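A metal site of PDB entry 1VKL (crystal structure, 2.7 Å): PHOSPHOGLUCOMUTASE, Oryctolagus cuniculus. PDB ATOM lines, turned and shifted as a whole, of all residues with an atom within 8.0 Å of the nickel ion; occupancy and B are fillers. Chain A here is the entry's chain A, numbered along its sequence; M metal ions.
The side-chain carboxylate (OD2) of Asp 287 is in hydrogen-bond range of the backbone NH (N) of Gly 290, 3.3 Å away.
The side-chain amino group of Lys 388 lies within salt-bridge range of the side-chain carboxylate of Asp 291 (2.8 Å).
OD1 of Asp 289 lies within hydrogen-bond range of OG1 of Thr 95.
O of SEP 116 is in hydrogen-bond range of the guanidinium group of Arg 63 (2.8 Å).
The backbone NH (N) of Arg 292 lies within hydrogen-bond range of the side-chain carboxylate (OD2) of Asp 287 (2.9 Å).
O1P of SEP 116 lies within salt-bridge range of NH2 of Arg 292.
O1P of SEP 116 lies within hydrogen-bond range of ND1 of His 117 (2.6 Å).
The side-chain hydroxyl (OG1) of Thr 114 is in hydrogen-bond range of N of SEP 116 (3.1 Å).
The nickel ion is bound by OD1 of Asp 287, OD2 of Asp 289, O2P of SEP 116 and OD1 of Asp 291.
The nickel ion has four donor atoms within binding distance.
Of the 25 residues printed, 4 come within 4 Å of the nickel ion.
The nearest printed residue that does not touch the nickel ion is Arg 292 (4.4 Å).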
ATOM      1  N   ARG A  22      10.823  30.335   0.695  1.00  0.00           N
ATOM      2  CA  ARG A  22      10.023  29.122   1.039  1.00  0.00           C
ATOM      3  C   ARG A  22       9.360  29.298   2.390  1.00  0.00           C
ATOM      4  O   ARG A  22       9.955  29.794   3.371  1.00  0.00           O
ATOM      5  CB  ARG A  22      10.765  27.768   1.240  1.00  0.00           C
ATOM      6  CG  ARG A  22      11.997  27.661   0.378  1.00  0.00           C
ATOM      7  CD  ARG A  22      12.040  26.441  -0.542  1.00  0.00           C
ATOM      8  NE  ARG A  22      12.413  26.856  -1.901  1.00  0.00           N
ATOM      9  CZ  ARG A  22      13.151  26.140  -2.721  1.00  0.00           C
ATOM     10  NH1 ARG A  22      13.653  24.958  -2.359  1.00  0.00           N
ATOM     11  NH2 ARG A  22      13.361  26.632  -3.911  1.00  0.00           N
ATOM     12  N   ASP A  61       7.094  22.236  -9.788  1.00  0.00           N
ATOM     13  CA  ASP A  61       7.161  20.791  -9.606  1.00  0.00           C
ATOM     14  C   ASP A  61       5.830  20.082  -9.468  1.00  0.00           C
ATOM     15  O   ASP A  61       5.702  18.847  -9.326  1.00  0.00           O
ATOM     16  CB  ASP A  61       8.049  20.507  -8.404  1.00  0.00           C
ATOM     17  CG  ASP A  61       7.644  21.179  -7.101  1.00  0.00           C
ATOM     18  OD1 ASP A  61       6.570  21.768  -7.014  1.00  0.00           O
ATOM     19  OD2 ASP A  61       8.412  21.117  -6.145  1.00  0.00           O
ATOM     20  N   ARG A  63       3.486  20.542  -6.998  1.00  0.00           N
ATOM     21  CA  ARG A  63       2.920  20.350  -5.672  1.00  0.00           C
ATOM     22  C   ARG A  63       1.631  21.174  -5.471  1.00  0.00           C
ATOM     23  O   ARG A  63       1.354  22.104  -6.241  1.00  0.00           O
ATOM     24  CB  ARG A  63       3.955  20.758  -4.651  1.00  0.00           C
ATOM     25  CG  ARG A  63       4.308  22.250  -4.700  1.00  0.00           C
ATOM     26  CD  ARG A  63       5.438  22.615  -3.768  1.00  0.00           C
ATOM     27  NE  ARG A  63       6.644  21.830  -3.992  1.00  0.00           N
ATOM     28  CZ  ARG A  63       7.357  21.236  -3.041  1.00  0.00           C
ATOM     29  NH1 ARG A  63       7.000  21.314  -1.784  1.00  0.00           N
ATOM     30  NH2 ARG A  63       8.480  20.614  -3.378  1.00  0.00           N
ATOM     31  N   THR A  95      13.007  22.126 -12.851  1.00  0.00           N
ATOM     32  CA  THR A  95      13.974  23.215 -12.729  1.00  0.00           C
ATOM     33  C   THR A  95      14.965  23.145 -13.876  1.00  0.00           C
ATOM     34  O   THR A  95      15.208  24.201 -14.471  1.00  0.00           O
ATOM     35  CB  THR A  95      14.713  23.191 -11.379  1.00  0.00           C
ATOM     36  OG1 THR A  95      13.682  23.688 -10.550  1.00  0.00           O
ATOM     37  CG2 THR A  95      15.946  24.069 -11.198  1.00  0.00           C
ATOM     38  N   PRO A  96      15.525  22.020 -14.305  1.00  0.00           N
ATOM     39  CA  PRO A  96      16.432  21.933 -15.450  1.00  0.00           C
ATOM     40  C   PRO A  96      15.693  22.425 -16.738  1.00  0.00           C
ATOM     41  O   PRO A  96      16.255  23.155 -17.569  1.00  0.00           O
ATOM     42  CB  PRO A  96      16.782  20.512 -15.573  1.00  0.00           C
ATOM     43  CG  PRO A  96      16.809  20.087 -14.135  1.00  0.00           C
ATOM     44  CD  PRO A  96      15.596  20.792 -13.547  1.00  0.00           C
ATOM     45  N   THR A 114       8.595  25.796  -6.777  1.00  0.00           N
ATOM     46  CA  THR A 114       9.049  24.525  -6.166  1.00  0.00           C
ATOM     47  C   THR A 114       9.677  24.694  -4.740  1.00  0.00           C
ATOM     48  O   THR A 114      10.165  25.788  -4.382  1.00  0.00           O
ATOM     49  CB  THR A 114      10.109  23.862  -7.094  1.00  0.00           C
ATOM     50  OG1 THR A 114      10.529  22.641  -6.517  1.00  0.00           O
ATOM     51  CG2 THR A 114      11.350  24.736  -7.243  1.00  0.00           C
ATOM     52  N   ALA A 115       9.633  23.708  -3.829  1.00  0.00           N
ATOM     53  CA  ALA A 115      10.296  23.793  -2.513  1.00  0.00           C
ATOM     54  C   ALA A 115      11.209  22.561  -2.515  1.00  0.00           C
ATOM     55  O   ALA A 115      11.475  21.970  -1.481  1.00  0.00           O
ATOM     56  CB  ALA A 115       9.324  23.713  -1.312  1.00  0.00           C
ATOM     57  N   SEP A 116      11.723  22.175  -3.692  1.00  0.00           N
ATOM     58  CA  SEP A 116      12.593  21.049  -4.024  1.00  0.00           C
ATOM     59  CB  SEP A 116      14.127  21.429  -3.744  1.00  0.00           C
ATOM     60  OG  SEP A 116      14.902  20.258  -3.483  1.00  0.00           O
ATOM     61  C   SEP A 116      12.159  19.783  -3.283  1.00  0.00           C
ATOM     62  O   SEP A 116      10.978  19.441  -3.438  1.00  0.00           O
ATOM     63  P   SEP A 116      16.331  20.592  -3.229  1.00  0.00           P
ATOM     64  O1P SEP A 116      16.862  19.642  -2.195  1.00  0.00           O
ATOM     65  O2P SEP A 116      17.092  20.416  -4.484  1.00  0.00           O
ATOM     66  O3P SEP A 116      16.457  21.998  -2.726  1.00  0.00           O
ATOM     67  N   HIS A 117      12.926  19.047  -2.478  1.00  0.00           N
ATOM     68  CA  HIS A 117      12.531  17.855  -1.748  1.00  0.00           C
ATOM     69  C   HIS A 117      11.603  18.109  -0.542  1.00  0.00           C
ATOM     70  O   HIS A 117      11.130  17.201   0.152  1.00  0.00           O
ATOM     71  CB  HIS A 117      13.813  17.134  -1.284  1.00  0.00           C
ATOM     72  CG  HIS A 117      14.463  17.986  -0.209  1.00  0.00           C
ATOM     73  ND1 HIS A 117      15.009  19.165  -0.431  1.00  0.00           N
ATOM     74  CD2 HIS A 117      14.502  17.707   1.142  1.00  0.00           C
ATOM     75  CE1 HIS A 117      15.358  19.639   0.720  1.00  0.00           C
ATOM     76  NE2 HIS A 117      15.058  18.761   1.661  1.00  0.00           N
ATOM     77  N   ASN A 118      11.400  19.360  -0.186  1.00  0.00           N
ATOM     78  CA  ASN A 118      10.495  19.692   0.905  1.00  0.00           C
ATOM     79  C   ASN A 118       9.081  19.307   0.517  1.00  0.00           C
ATOM     80  O   ASN A 118       8.599  19.644  -0.560  1.00  0.00           O
ATOM     81  CB  ASN A 118      10.426  21.161   1.221  1.00  0.00           C
ATOM     82  CG  ASN A 118      11.720  21.738   1.721  1.00  0.00           C
ATOM     83  OD1 ASN A 118      12.742  21.091   1.843  1.00  0.00           O
ATOM     84  ND2 ASN A 118      11.712  23.001   2.059  1.00  0.00           N
ATOM     85  N   LYS A 129      10.980  30.412  -6.364  1.00  0.00           N
ATOM     86  CA  LYS A 129      12.337  30.707  -6.785  1.00  0.00           C
ATOM     87  C   LYS A 129      12.409  31.607  -8.033  1.00  0.00           C
ATOM     88  O   LYS A 129      11.656  31.395  -8.977  1.00  0.00           O
ATOM     89  CB  LYS A 129      13.057  29.381  -7.033  1.00  0.00           C
ATOM     90  CG  LYS A 129      14.514  29.402  -7.473  1.00  0.00           C
ATOM     91  CD  LYS A 129      14.712  27.918  -7.634  1.00  0.00           C
ATOM     92  CE  LYS A 129      16.106  27.545  -8.013  1.00  0.00           C
ATOM     93  NZ  LYS A 129      16.277  27.640  -9.435  1.00  0.00           N
ATOM     94  N   PRO A 261       9.902  13.842  -1.565  1.00  0.00           N
ATOM     95  CA  PRO A 261      10.625  13.444  -2.781  1.00  0.00           C
ATOM     96  C   PRO A 261      12.112  13.677  -2.543  1.00  0.00           C
ATOM     97  O   PRO A 261      12.688  14.617  -3.096  1.00  0.00           O
ATOM     98  CB  PRO A 261      10.017  14.298  -3.850  1.00  0.00           C
ATOM     99  CG  PRO A 261       9.765  15.606  -3.097  1.00  0.00           C
ATOM    100  CD  PRO A 261       9.243  15.140  -1.770  1.00  0.00           C
ATOM    101  N   ASP A 262      12.719  12.934  -1.623  1.00  0.00           N
ATOM    102  CA  ASP A 262      14.117  13.157  -1.395  1.00  0.00           C
ATOM    103  C   ASP A 262      14.957  11.952  -1.783  1.00  0.00           C
ATOM    104  O   ASP A 262      14.946  10.870  -1.165  1.00  0.00           O
ATOM    105  CB  ASP A 262      14.347  13.523   0.046  1.00  0.00           C
ATOM    106  CG  ASP A 262      15.617  14.343   0.272  1.00  0.00           C
ATOM    107  OD1 ASP A 262      15.770  14.821   1.383  1.00  0.00           O
ATOM    108  OD2 ASP A 262      16.434  14.575  -0.618  1.00  0.00           O
ATOM    109  N   PRO A 263      15.727  12.137  -2.863  1.00  0.00           N
ATOM    110  CA  PRO A 263      16.574  11.102  -3.408  1.00  0.00           C
ATOM    111  C   PRO A 263      17.685  10.555  -2.534  1.00  0.00           C
ATOM    112  O   PRO A 263      18.820  11.029  -2.595  1.00  0.00           O
ATOM    113  CB  PRO A 263      17.040  11.733  -4.715  1.00  0.00           C
ATOM    114  CG  PRO A 263      17.226  13.159  -4.370  1.00  0.00           C
ATOM    115  CD  PRO A 263      15.982  13.395  -3.571  1.00  0.00           C
ATOM    116  N   PHE A 286      14.862  10.718  -8.275  1.00  0.00           N
ATOM    117  CA  PHE A 286      15.118  12.150  -8.416  1.00  0.00           C
ATOM    118  C   PHE A 286      14.312  12.892  -7.371  1.00  0.00           C
ATOM    119  O   PHE A 286      13.460  12.279  -6.729  1.00  0.00           O
ATOM    120  CB  PHE A 286      14.681  12.739  -9.750  1.00  0.00           C
ATOM    121  CG  PHE A 286      15.137  11.978 -10.971  1.00  0.00           C
ATOM    122  CD1 PHE A 286      14.295  10.986 -11.514  1.00  0.00           C
ATOM    123  CD2 PHE A 286      16.361  12.243 -11.556  1.00  0.00           C
ATOM    124  CE1 PHE A 286      14.695  10.256 -12.624  1.00  0.00           C
ATOM    125  CE2 PHE A 286      16.745  11.499 -12.680  1.00  0.00           C
ATOM    126  CZ  PHE A 286      15.916  10.510 -13.216  1.00  0.00           C
ATOM    127  N   ASP A 287      14.548  14.175  -7.126  1.00  0.00           N
ATOM    128  CA  ASP A 287      13.804  14.958  -6.146  1.00  0.00           C
ATOM    129  C   ASP A 287      12.589  15.694  -6.748  1.00  0.00           C
ATOM    130  O   ASP A 287      12.296  15.584  -7.950  1.00  0.00           O
ATOM    131  CB  ASP A 287      14.796  15.932  -5.511  1.00  0.00           C
ATOM    132  CG  ASP A 287      15.273  17.009  -6.458  1.00  0.00           C
ATOM    133  OD1 ASP A 287      15.184  18.141  -6.079  1.00  0.00           O
ATOM    134  OD2 ASP A 287      15.668  16.698  -7.579  1.00  0.00           O
ATOM    135  N   GLY A 288      11.905  16.522  -5.955  1.00  0.00           N
ATOM    136  CA  GLY A 288      10.727  17.281  -6.335  1.00  0.00           C
ATOM    137  C   GLY A 288      10.873  18.028  -7.646  1.00  0.00           C
ATOM    138  O   GLY A 288      10.025  17.843  -8.530  1.00  0.00           O
ATOM    139  N   ASP A 289      11.956  18.793  -7.853  1.00  0.00           N
ATOM    140  CA  ASP A 289      12.083  19.513  -9.095  1.00  0.00           C
ATOM    141  C   ASP A 289      13.074  18.999 -10.157  1.00  0.00           C
ATOM    142  O   ASP A 289      13.334  19.591 -11.205  1.00  0.00           O
ATOM    143  CB  ASP A 289      12.303  20.977  -8.684  1.00  0.00           C
ATOM    144  CG  ASP A 289      13.594  21.353  -7.987  1.00  0.00           C
ATOM    145  OD1 ASP A 289      13.916  22.536  -8.064  1.00  0.00           O
ATOM    146  OD2 ASP A 289      14.237  20.508  -7.382  1.00  0.00           O
ATOM    147  N   GLY A 290      13.632  17.820  -9.937  1.00  0.00           N
ATOM    148  CA  GLY A 290      14.498  17.218 -10.931  1.00  0.00           C
ATOM    149  C   GLY A 290      15.940  17.648 -11.025  1.00  0.00           C
ATOM    150  O   GLY A 290      16.592  17.265 -12.022  1.00  0.00           O
ATOM    151  N   ASP A 291      16.487  18.394 -10.060  1.00  0.00           N
ATOM    152  CA  ASP A 291      17.881  18.736 -10.201  1.00  0.00           C
ATOM    153  C   ASP A 291      18.893  17.935  -9.367  1.00  0.00           C
ATOM    154  O   ASP A 291      20.122  18.047  -9.465  1.00  0.00           O
ATOM    155  CB  ASP A 291      17.891  20.233 -10.019  1.00  0.00           C
ATOM    156  CG  ASP A 291      18.130  20.880  -8.699  1.00  0.00           C
ATOM    157  OD1 ASP A 291      17.504  20.526  -7.692  1.00  0.00           O
ATOM    158  OD2 ASP A 291      18.987  21.768  -8.737  1.00  0.00           O
ATOM    159  N   ARG A 292      18.367  16.946  -8.644  1.00  0.00           N
ATOM    160  CA  ARG A 292      19.181  16.045  -7.856  1.00  0.00           C
ATOM    161  C   ARG A 292      18.827  14.593  -8.167  1.00  0.00           C
ATOM    162  O   ARG A 292      17.735  14.212  -8.606  1.00  0.00           O
ATOM    163  CB  ARG A 292      19.025  16.304  -6.336  1.00  0.00           C
ATOM    164  CG  ARG A 292      19.822  17.579  -5.885  1.00  0.00           C
ATOM    165  CD  ARG A 292      19.995  17.880  -4.396  1.00  0.00           C
ATOM    166  NE  ARG A 292      18.721  17.890  -3.712  1.00  0.00           N
ATOM    167  CZ  ARG A 292      18.338  16.954  -2.857  1.00  0.00           C
ATOM    168  NH1 ARG A 292      19.134  15.960  -2.596  1.00  0.00           N
ATOM    169  NH2 ARG A 292      17.153  17.023  -2.309  1.00  0.00           N
ATOM    170  N   ASN A 293      19.847  13.742  -7.991  1.00  0.00           N
ATOM    171  CA  ASN A 293      19.707  12.326  -8.267  1.00  0.00           C
ATOM    172  C   ASN A 293      20.477  11.337  -7.396  1.00  0.00           C
ATOM    173  O   ASN A 293      21.524  11.688  -6.846  1.00  0.00           O
ATOM    174  CB  ASN A 293      20.145  12.025  -9.713  1.00  0.00           C
ATOM    175  CG  ASN A 293      21.627  12.257  -9.966  1.00  0.00           C
ATOM    176  OD1 ASN A 293      22.211  13.348  -9.872  1.00  0.00           O
ATOM    177  ND2 ASN A 293      22.283  11.166 -10.329  1.00  0.00           N
ATOM    178  N   PHE A 378      23.704  14.474  -3.513  1.00  0.00           N
ATOM    179  CA  PHE A 378      23.005  13.964  -4.693  1.00  0.00           C
ATOM    180  C   PHE A 378      22.884  14.988  -5.828  1.00  0.00           C
ATOM    181  O   PHE A 378      21.883  15.134  -6.515  1.00  0.00           O
ATOM    182  CB  PHE A 378      21.636  13.451  -4.188  1.00  0.00           C
ATOM    183  CG  PHE A 378      21.841  12.290  -3.233  1.00  0.00           C
ATOM    184  CD1 PHE A 378      21.863  10.989  -3.740  1.00  0.00           C
ATOM    185  CD2 PHE A 378      22.040  12.520  -1.877  1.00  0.00           C
ATOM    186  CE1 PHE A 378      22.088   9.900  -2.877  1.00  0.00           C
ATOM    187  CE2 PHE A 378      22.271  11.439  -1.029  1.00  0.00           C
ATOM    188  CZ  PHE A 378      22.297  10.121  -1.522  1.00  0.00           C
ATOM    189  N   GLU A 387      21.714  25.196 -13.803  1.00  0.00           N
ATOM    190  CA  GLU A 387      21.042  24.534 -12.687  1.00  0.00           C
ATOM    191  C   GLU A 387      21.489  23.098 -12.600  1.00  0.00           C
ATOM    192  O   GLU A 387      22.013  22.569 -13.600  1.00  0.00           O
ATOM    193  CB  GLU A 387      19.574  24.381 -12.810  1.00  0.00           C
ATOM    194  CG  GLU A 387      18.777  25.647 -12.661  1.00  0.00           C
ATOM    195  CD  GLU A 387      18.618  26.206 -11.264  1.00  0.00           C
ATOM    196  OE1 GLU A 387      18.946  25.589 -10.233  1.00  0.00           O
ATOM    197  OE2 GLU A 387      18.079  27.300 -11.194  1.00  0.00           O
ATOM    198  N   LYS A 388      21.350  22.390 -11.477  1.00  0.00           N
ATOM    199  CA  LYS A 388      21.764  20.998 -11.543  1.00  0.00           C
ATOM    200  C   LYS A 388      20.673  20.250 -12.366  1.00  0.00           C
ATOM    201  O   LYS A 388      19.537  20.694 -12.569  1.00  0.00           O
ATOM    202  CB  LYS A 388      21.892  20.445 -10.119  1.00  0.00           C
ATOM    203  CG  LYS A 388      23.060  20.936  -9.232  1.00  0.00           C
ATOM    204  CD  LYS A 388      22.583  21.528  -7.893  1.00  0.00           C
ATOM    205  CE  LYS A 388      21.903  20.575  -6.917  1.00  0.00           C
ATOM    206  NZ  LYS A 388      20.564  21.066  -6.534  1.00  0.00           N
HETATM  207 NI    NI M   1      15.898  20.055  -6.216  1.00  0.00          NI
